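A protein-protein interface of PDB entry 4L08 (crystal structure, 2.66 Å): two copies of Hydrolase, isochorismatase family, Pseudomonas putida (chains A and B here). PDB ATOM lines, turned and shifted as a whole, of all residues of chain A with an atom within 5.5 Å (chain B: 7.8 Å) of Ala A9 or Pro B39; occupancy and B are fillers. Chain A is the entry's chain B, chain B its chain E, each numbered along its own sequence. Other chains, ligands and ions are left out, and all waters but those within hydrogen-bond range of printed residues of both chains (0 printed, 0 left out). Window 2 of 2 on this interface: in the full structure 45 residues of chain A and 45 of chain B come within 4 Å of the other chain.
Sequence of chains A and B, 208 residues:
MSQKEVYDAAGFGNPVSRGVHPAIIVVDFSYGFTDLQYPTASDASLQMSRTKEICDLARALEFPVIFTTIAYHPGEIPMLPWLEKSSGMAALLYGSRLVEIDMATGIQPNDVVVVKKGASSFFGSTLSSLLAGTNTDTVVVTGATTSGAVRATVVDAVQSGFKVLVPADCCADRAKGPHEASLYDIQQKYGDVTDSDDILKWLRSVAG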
ATOM      1  N   LYS A   4      -2.259  26.922  28.261  1.00  0.00           N
ATOM      2  CA  LYS A   4      -2.455  27.098  29.699  1.00  0.00           C
ATOM      3  C   LYS A   4      -3.763  27.829  29.979  1.00  0.00           C
ATOM      4  O   LYS A   4      -4.501  27.460  30.892  1.00  0.00           O
ATOM      5  CB  LYS A   4      -1.297  27.892  30.308  1.00  0.00           C
ATOM      6  CG  LYS A   4      -1.079  27.661  31.807  1.00  0.00           C
ATOM      7  CD  LYS A   4       0.267  26.970  32.076  1.00  0.00           C
ATOM      8  CE  LYS A   4       0.267  25.477  31.706  1.00  0.00           C
ATOM      9  NZ  LYS A   4       1.529  24.812  32.189  1.00  0.00           N
ATOM     10  N   GLU A   5      -4.037  28.863  29.185  1.00  0.00           N
ATOM     11  CA  GLU A   5      -5.261  29.655  29.306  1.00  0.00           C
ATOM     12  C   GLU A   5      -6.512  28.850  28.941  1.00  0.00           C
ATOM     13  O   GLU A   5      -7.568  29.027  29.555  1.00  0.00           O
ATOM     14  CB  GLU A   5      -5.162  30.917  28.454  1.00  0.00           C
ATOM     15  N   VAL A   6      -6.380  27.970  27.949  1.00  0.00           N
ATOM     16  CA  VAL A   6      -7.478  27.108  27.501  1.00  0.00           C
ATOM     17  C   VAL A   6      -7.905  26.135  28.601  1.00  0.00           C
ATOM     18  O   VAL A   6      -9.099  25.959  28.856  1.00  0.00           O
ATOM     19  CB  VAL A   6      -7.103  26.315  26.224  1.00  0.00           C
ATOM     20  CG1 VAL A   6      -8.259  25.428  25.770  1.00  0.00           C
ATOM     21  CG2 VAL A   6      -6.693  27.260  25.100  1.00  0.00           C
ATOM     22  N   TYR A   7      -6.920  25.516  29.250  1.00  0.00           N
ATOM     23  CA  TYR A   7      -7.173  24.518  30.288  1.00  0.00           C
ATOM     24  C   TYR A   7      -7.671  25.126  31.600  1.00  0.00           C
ATOM     25  O   TYR A   7      -8.485  24.517  32.299  1.00  0.00           O
ATOM     26  CB  TYR A   7      -5.924  23.660  30.523  1.00  0.00           C
ATOM     27  CG  TYR A   7      -5.775  22.504  29.550  1.00  0.00           C
ATOM     28  CD1 TYR A   7      -6.279  21.239  29.858  1.00  0.00           C
ATOM     29  CD2 TYR A   7      -5.126  22.673  28.324  1.00  0.00           C
ATOM     30  CE1 TYR A   7      -6.145  20.179  28.974  1.00  0.00           C
ATOM     31  CE2 TYR A   7      -4.987  21.618  27.433  1.00  0.00           C
ATOM     32  CZ  TYR A   7      -5.498  20.373  27.762  1.00  0.00           C
ATOM     33  OH  TYR A   7      -5.363  19.321  26.880  1.00  0.00           O
ATOM     34  N   ASP A   8      -7.190  26.325  31.921  1.00  0.00           N
ATOM     35  CA  ASP A   8      -7.595  27.027  33.146  1.00  0.00           C
ATOM     36  C   ASP A   8      -9.034  27.548  33.088  1.00  0.00           C
ATOM     37  O   ASP A   8      -9.726  27.581  34.109  1.00  0.00           O
ATOM     38  CB  ASP A   8      -6.620  28.169  33.466  1.00  0.00           C
ATOM     39  CG  ASP A   8      -5.240  27.667  33.886  1.00  0.00           C
ATOM     40  OD1 ASP A   8      -5.071  26.441  34.078  1.00  0.00           O
ATOM     41  OD2 ASP A   8      -4.318  28.504  34.022  1.00  0.00           O
ATOM     42  N   ALA A   9      -9.469  27.955  31.894  1.00  0.00           N
ATOM     43  CA  ALA A   9     -10.846  28.403  31.662  1.00  0.00           C
ATOM     44  C   ALA A   9     -11.813  27.223  31.604  1.00  0.00           C
ATOM     45  O   ALA A   9     -12.960  27.327  32.044  1.00  0.00           O
ATOM     46  CB  ALA A   9     -10.932  29.227  30.388  1.00  0.00           C
ATOM     47  N   ALA A  10     -11.338  26.101  31.065  1.00  0.00           N
ATOM     48  CA  ALA A  10     -12.103  24.855  31.053  1.00  0.00           C
ATOM     49  C   ALA A  10     -12.190  24.237  32.452  1.00  0.00           C
ATOM     50  O   ALA A  10     -12.902  23.253  32.664  1.00  0.00           O
ATOM     51  CB  ALA A  10     -11.496  23.870  30.063  1.00  0.00           C
ATOM     52  N   GLY A  11     -11.456  24.823  33.397  1.00  0.00           N
ATOM     53  CA  GLY A  11     -11.521  24.431  34.801  1.00  0.00           C
ATOM     54  C   GLY A  11     -10.685  23.214  35.149  1.00  0.00           C
ATOM     55  O   GLY A  11     -11.067  22.425  36.016  1.00  0.00           O
ATOM     56  N   GLY B  32     -21.644  20.838  25.165  1.00  0.00           N
ATOM     57  CA  GLY B  32     -20.642  21.217  26.162  1.00  0.00           C
ATOM     58  C   GLY B  32     -19.204  21.066  25.691  1.00  0.00           C
ATOM     59  O   GLY B  32     -18.307  21.744  26.199  1.00  0.00           O
ATOM     60  N   PHE B  33     -18.987  20.186  24.716  1.00  0.00           N
ATOM     61  CA  PHE B  33     -17.649  19.940  24.176  1.00  0.00           C
ATOM     62  C   PHE B  33     -17.484  20.388  22.720  1.00  0.00           C
ATOM     63  O   PHE B  33     -16.365  20.400  22.197  1.00  0.00           O
ATOM     64  CB  PHE B  33     -17.269  18.462  24.338  1.00  0.00           C
ATOM     65  CG  PHE B  33     -17.287  17.986  25.763  1.00  0.00           C
ATOM     66  CD1 PHE B  33     -16.199  18.216  26.603  1.00  0.00           C
ATOM     67  CD2 PHE B  33     -18.396  17.317  26.271  1.00  0.00           C
ATOM     68  CE1 PHE B  33     -16.219  17.787  27.920  1.00  0.00           C
ATOM     69  CE2 PHE B  33     -18.422  16.884  27.587  1.00  0.00           C
ATOM     70  CZ  PHE B  33     -17.333  17.121  28.412  1.00  0.00           C
ATOM     71  N   ASP B  35     -19.742  23.236  21.201  1.00  0.00           N
ATOM     72  CA  ASP B  35     -20.150  24.633  21.014  1.00  0.00           C
ATOM     73  C   ASP B  35     -19.166  25.584  21.699  1.00  0.00           C
ATOM     74  O   ASP B  35     -19.071  25.613  22.928  1.00  0.00           O
ATOM     75  CB  ASP B  35     -21.575  24.857  21.536  1.00  0.00           C
ATOM     76  CG  ASP B  35     -22.247  26.085  20.926  1.00  0.00           C
ATOM     77  OD1 ASP B  35     -21.650  27.186  20.953  1.00  0.00           O
ATOM     78  OD2 ASP B  35     -23.392  25.945  20.429  1.00  0.00           O
ATOM     79  N   LEU B  36     -18.463  26.378  20.893  1.00  0.00           N
ATOM     80  CA  LEU B  36     -17.345  27.205  21.369  1.00  0.00           C
ATOM     81  C   LEU B  36     -17.717  28.384  22.284  1.00  0.00           C
ATOM     82  O   LEU B  36     -16.831  29.084  22.795  1.00  0.00           O
ATOM     83  CB  LEU B  36     -16.479  27.682  20.193  1.00  0.00           C
ATOM     84  CG  LEU B  36     -15.795  26.577  19.371  1.00  0.00           C
ATOM     85  CD1 LEU B  36     -16.608  26.245  18.124  1.00  0.00           C
ATOM     86  CD2 LEU B  36     -14.373  26.993  18.990  1.00  0.00           C
ATOM     87  N   GLN B  37     -19.018  28.594  22.501  1.00  0.00           N
ATOM     88  CA  GLN B  37     -19.471  29.582  23.481  1.00  0.00           C
ATOM     89  C   GLN B  37     -19.117  29.137  24.909  1.00  0.00           C
ATOM     90  O   GLN B  37     -19.061  29.958  25.827  1.00  0.00           O
ATOM     91  CB  GLN B  37     -20.976  29.873  23.337  1.00  0.00           C
ATOM     92  CG  GLN B  37     -21.913  28.803  23.892  1.00  0.00           C
ATOM     93  CD  GLN B  37     -23.375  29.222  23.868  1.00  0.00           C
ATOM     94  OE1 GLN B  37     -23.944  29.580  24.901  1.00  0.00           O
ATOM     95  NE2 GLN B  37     -23.987  29.182  22.688  1.00  0.00           N
ATOM     96  N   TYR B  38     -18.870  27.837  25.074  1.00  0.00           N
ATOM     97  CA  TYR B  38     -18.503  27.255  26.365  1.00  0.00           C
ATOM     98  C   TYR B  38     -16.991  27.029  26.467  1.00  0.00           C
ATOM     99  O   TYR B  38     -16.361  26.606  25.494  1.00  0.00           O
ATOM    100  CB  TYR B  38     -19.245  25.933  26.591  1.00  0.00           C
ATOM    101  CG  TYR B  38     -20.747  26.009  26.412  1.00  0.00           C
ATOM    102  CD1 TYR B  38     -21.525  26.868  27.194  1.00  0.00           C
ATOM    103  CD2 TYR B  38     -21.393  25.207  25.472  1.00  0.00           C
ATOM    104  CE1 TYR B  38     -22.900  26.937  27.031  1.00  0.00           C
ATOM    105  CE2 TYR B  38     -22.768  25.262  25.306  1.00  0.00           C
ATOM    106  CZ  TYR B  38     -23.516  26.127  26.085  1.00  0.00           C
ATOM    107  OH  TYR B  38     -24.882  26.178  25.922  1.00  0.00           O
ATOM    108  N   PRO B  39     -16.408  27.304  27.654  1.00  0.00           N
ATOM    109  CA  PRO B  39     -14.962  27.169  27.878  1.00  0.00           C
ATOM    110  C   PRO B  39     -14.443  25.723  27.835  1.00  0.00           C
ATOM    111  O   PRO B  39     -13.260  25.504  27.551  1.00  0.00           O
ATOM    112  CB  PRO B  39     -14.773  27.761  29.279  1.00  0.00           C
ATOM    113  CG  PRO B  39     -16.094  27.579  29.949  1.00  0.00           C
ATOM    114  CD  PRO B  39     -17.104  27.792  28.863  1.00  0.00           C
ATOM    115  N   THR B  40     -15.322  24.756  28.111  1.00  0.00           N
ATOM    116  CA  THR B  40     -14.972  23.328  28.088  1.00  0.00           C
ATOM    117  C   THR B  40     -14.894  22.748  26.668  1.00  0.00           C
ATOM    118  O   THR B  40     -14.398  21.635  26.469  1.00  0.00           O
ATOM    119  CB  THR B  40     -15.971  22.482  28.912  1.00  0.00           C
ATOM    120  OG1 THR B  40     -17.306  22.731  28.459  1.00  0.00           O
ATOM    121  CG2 THR B  40     -15.879  22.814  30.394  1.00  0.00           C
ATOM    122  N   ALA B  41     -15.377  23.510  25.690  1.00  0.00           N
ATOM    123  CA  ALA B  41     -15.501  23.034  24.314  1.00  0.00           C
ATOM    124  C   ALA B  41     -14.251  23.258  23.468  1.00  0.00           C
ATOM    125  O   ALA B  41     -13.293  23.899  23.902  1.00  0.00           O
ATOM    126  CB  ALA B  41     -16.711  23.669  23.651  1.00  0.00           C
ATOM    127  N   SER B  42     -14.285  22.709  22.255  1.00  0.00           N
ATOM    128  CA  SER B  42     -13.204  22.814  21.275  1.00  0.00           C
ATOM    129  C   SER B  42     -13.784  22.597  19.875  1.00  0.00           C
ATOM    130  O   SER B  42     -14.818  21.938  19.730  1.00  0.00           O
ATOM    131  CB  SER B  42     -12.115  21.779  21.565  1.00  0.00           C
ATOM    132  OG  SER B  42     -12.669  20.481  21.720  1.00  0.00           O
ATOM    133  N   SER B  87     -13.079  21.032  37.571  1.00  0.00           N
ATOM    134  CA  SER B  87     -14.219  21.791  38.090  1.00  0.00           C
ATOM    135  C   SER B  87     -15.212  22.216  37.012  1.00  0.00           C
ATOM    136  O   SER B  87     -16.403  22.377  37.292  1.00  0.00           O
ATOM    137  CB  SER B  87     -13.734  23.013  38.875  1.00  0.00           C
ATOM    138  OG  SER B  87     -12.958  23.874  38.055  1.00  0.00           O
ATOM    139  N   GLY B  88     -14.721  22.386  35.785  1.00  0.00           N
ATOM    140  CA  GLY B  88     -15.550  22.812  34.658  1.00  0.00           C
ATOM    141  C   GLY B  88     -16.603  21.798  34.243  1.00  0.00           C
ATOM    142  O   GLY B  88     -17.603  22.152  33.609  1.00  0.00           O
ATOM    143  N   ALA B  91     -20.544  21.959  35.217  1.00  0.00           N
ATOM    144  CA  ALA B  91     -21.534  22.699  34.433  1.00  0.00           C
ATOM    145  C   ALA B  91     -22.442  21.767  33.624  1.00  0.00           C
ATOM    146  O   ALA B  91     -23.529  22.160  33.195  1.00  0.00           O
ATOM    147  CB  ALA B  91     -20.842  23.701  33.518  1.00  0.00           C
ATOM    148  N   LEU B  98     -25.819  21.896  27.495  1.00  0.00           N
ATOM    149  CA  LEU B  98     -24.470  21.329  27.373  1.00  0.00           C
ATOM    150  C   LEU B  98     -24.481  19.801  27.296  1.00  0.00           C
ATOM    151  O   LEU B  98     -23.565  19.199  26.735  1.00  0.00           O
ATOM    152  CB  LEU B  98     -23.548  21.776  28.522  1.00  0.00           C
ATOM    153  CG  LEU B  98     -23.720  23.022  29.405  1.00  0.00           C
ATOM    154  CD1 LEU B  98     -22.411  23.309  30.125  1.00  0.00           C
ATOM    155  CD2 LEU B  98     -24.170  24.259  28.649  1.00  0.00           C
ATOM    156  N   ARG B 174      -8.768  19.913  22.608  1.00  0.00           N
ATOM    157  CA  ARG B 174      -8.554  21.345  22.838  1.00  0.00           C
ATOM    158  C   ARG B 174      -7.117  21.811  22.573  1.00  0.00           C
ATOM    159  O   ARG B 174      -6.862  23.011  22.456  1.00  0.00           O
ATOM    160  CB  ARG B 174      -9.018  21.755  24.241  1.00  0.00           C
ATOM    161  CG  ARG B 174      -8.536  20.852  25.363  1.00  0.00           C
ATOM    162  CD  ARG B 174      -9.058  21.318  26.713  1.00  0.00           C
ATOM    163  NE  ARG B 174     -10.497  21.108  26.874  1.00  0.00           N
ATOM    164  CZ  ARG B 174     -11.055  19.972  27.288  1.00  0.00           C
ATOM    165  NH1 ARG B 174     -10.305  18.915  27.577  1.00  0.00           N
ATOM    166  NH2 ARG B 174     -12.373  19.890  27.411  1.00  0.00           N
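The backbone NH of Ser B87 sits at hydrogen-bond distance from the backbone carbonyl oxygen of Gly A11.
The backbone carbonyl oxygen of Gly B32 is in hydrogen-bond range of the side-chain hydroxyl of Thr B40, 2.7 Å away. NH2 of Arg B174 is in hydrogen-bond range of O of Thr B40.
Tyr A7 touches Arg B174. CB of Pro B39 touches O of Ala A9, 3.3 Å away. O of Pro B39 touches CB of Ala A10 (3.5 Å). Ala A10 touches Thr B40 (O to CG2, 3.8 Å). O of Ala A10 touches CA of Gly B88 (3.3 Å). Gly B88 touches Gly A11 (N to O, 3.7 Å).
Printed residues of chain A within 4 Å of Pro B39: Ala A9 (3.3 Å) and Ala A10 (3.5 Å). Of the printed residues of chain A, Ser B87 touches Gly A11 (2.9 Å). Of the printed residues of chain A, Gly B88 touches Ala A10 (3.3 Å) and Gly A11 (3.7 Å). Of the printed residues of chain B, Ala A10 touches Pro B39 (3.5 Å), Thr B40 (3.8 Å) and Gly B88 (3.3 Å). Printed residues of chain B within 4 Å of Gly A11: Ser B87 and Gly B88. The nearest residue of chain B that does not touch Ala A9 is Thr B40 (5.3 Å). The nearest residue of chain A that does not touch Pro B39 is Val A6 (4.4 Å).
Hydrophobic or aromatic side chains of chain A that line the printed part of chain B: Tyr A7 and Ala A10. Hydrophobic or aromatic side chains of chain B that line the printed part of chain A: Pro B39. Among the printed residues, 7 pairs touch across the chains. Among the printed residues, no Asp or Glu carboxylate lies within 4 Å of a Lys or Arg side-chain nitrogen of the other chain.
No position is printed for both chains. Of the 7 pairs that touch across the chains among the printed residues, none has its exchanged pair printed and touching as well.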
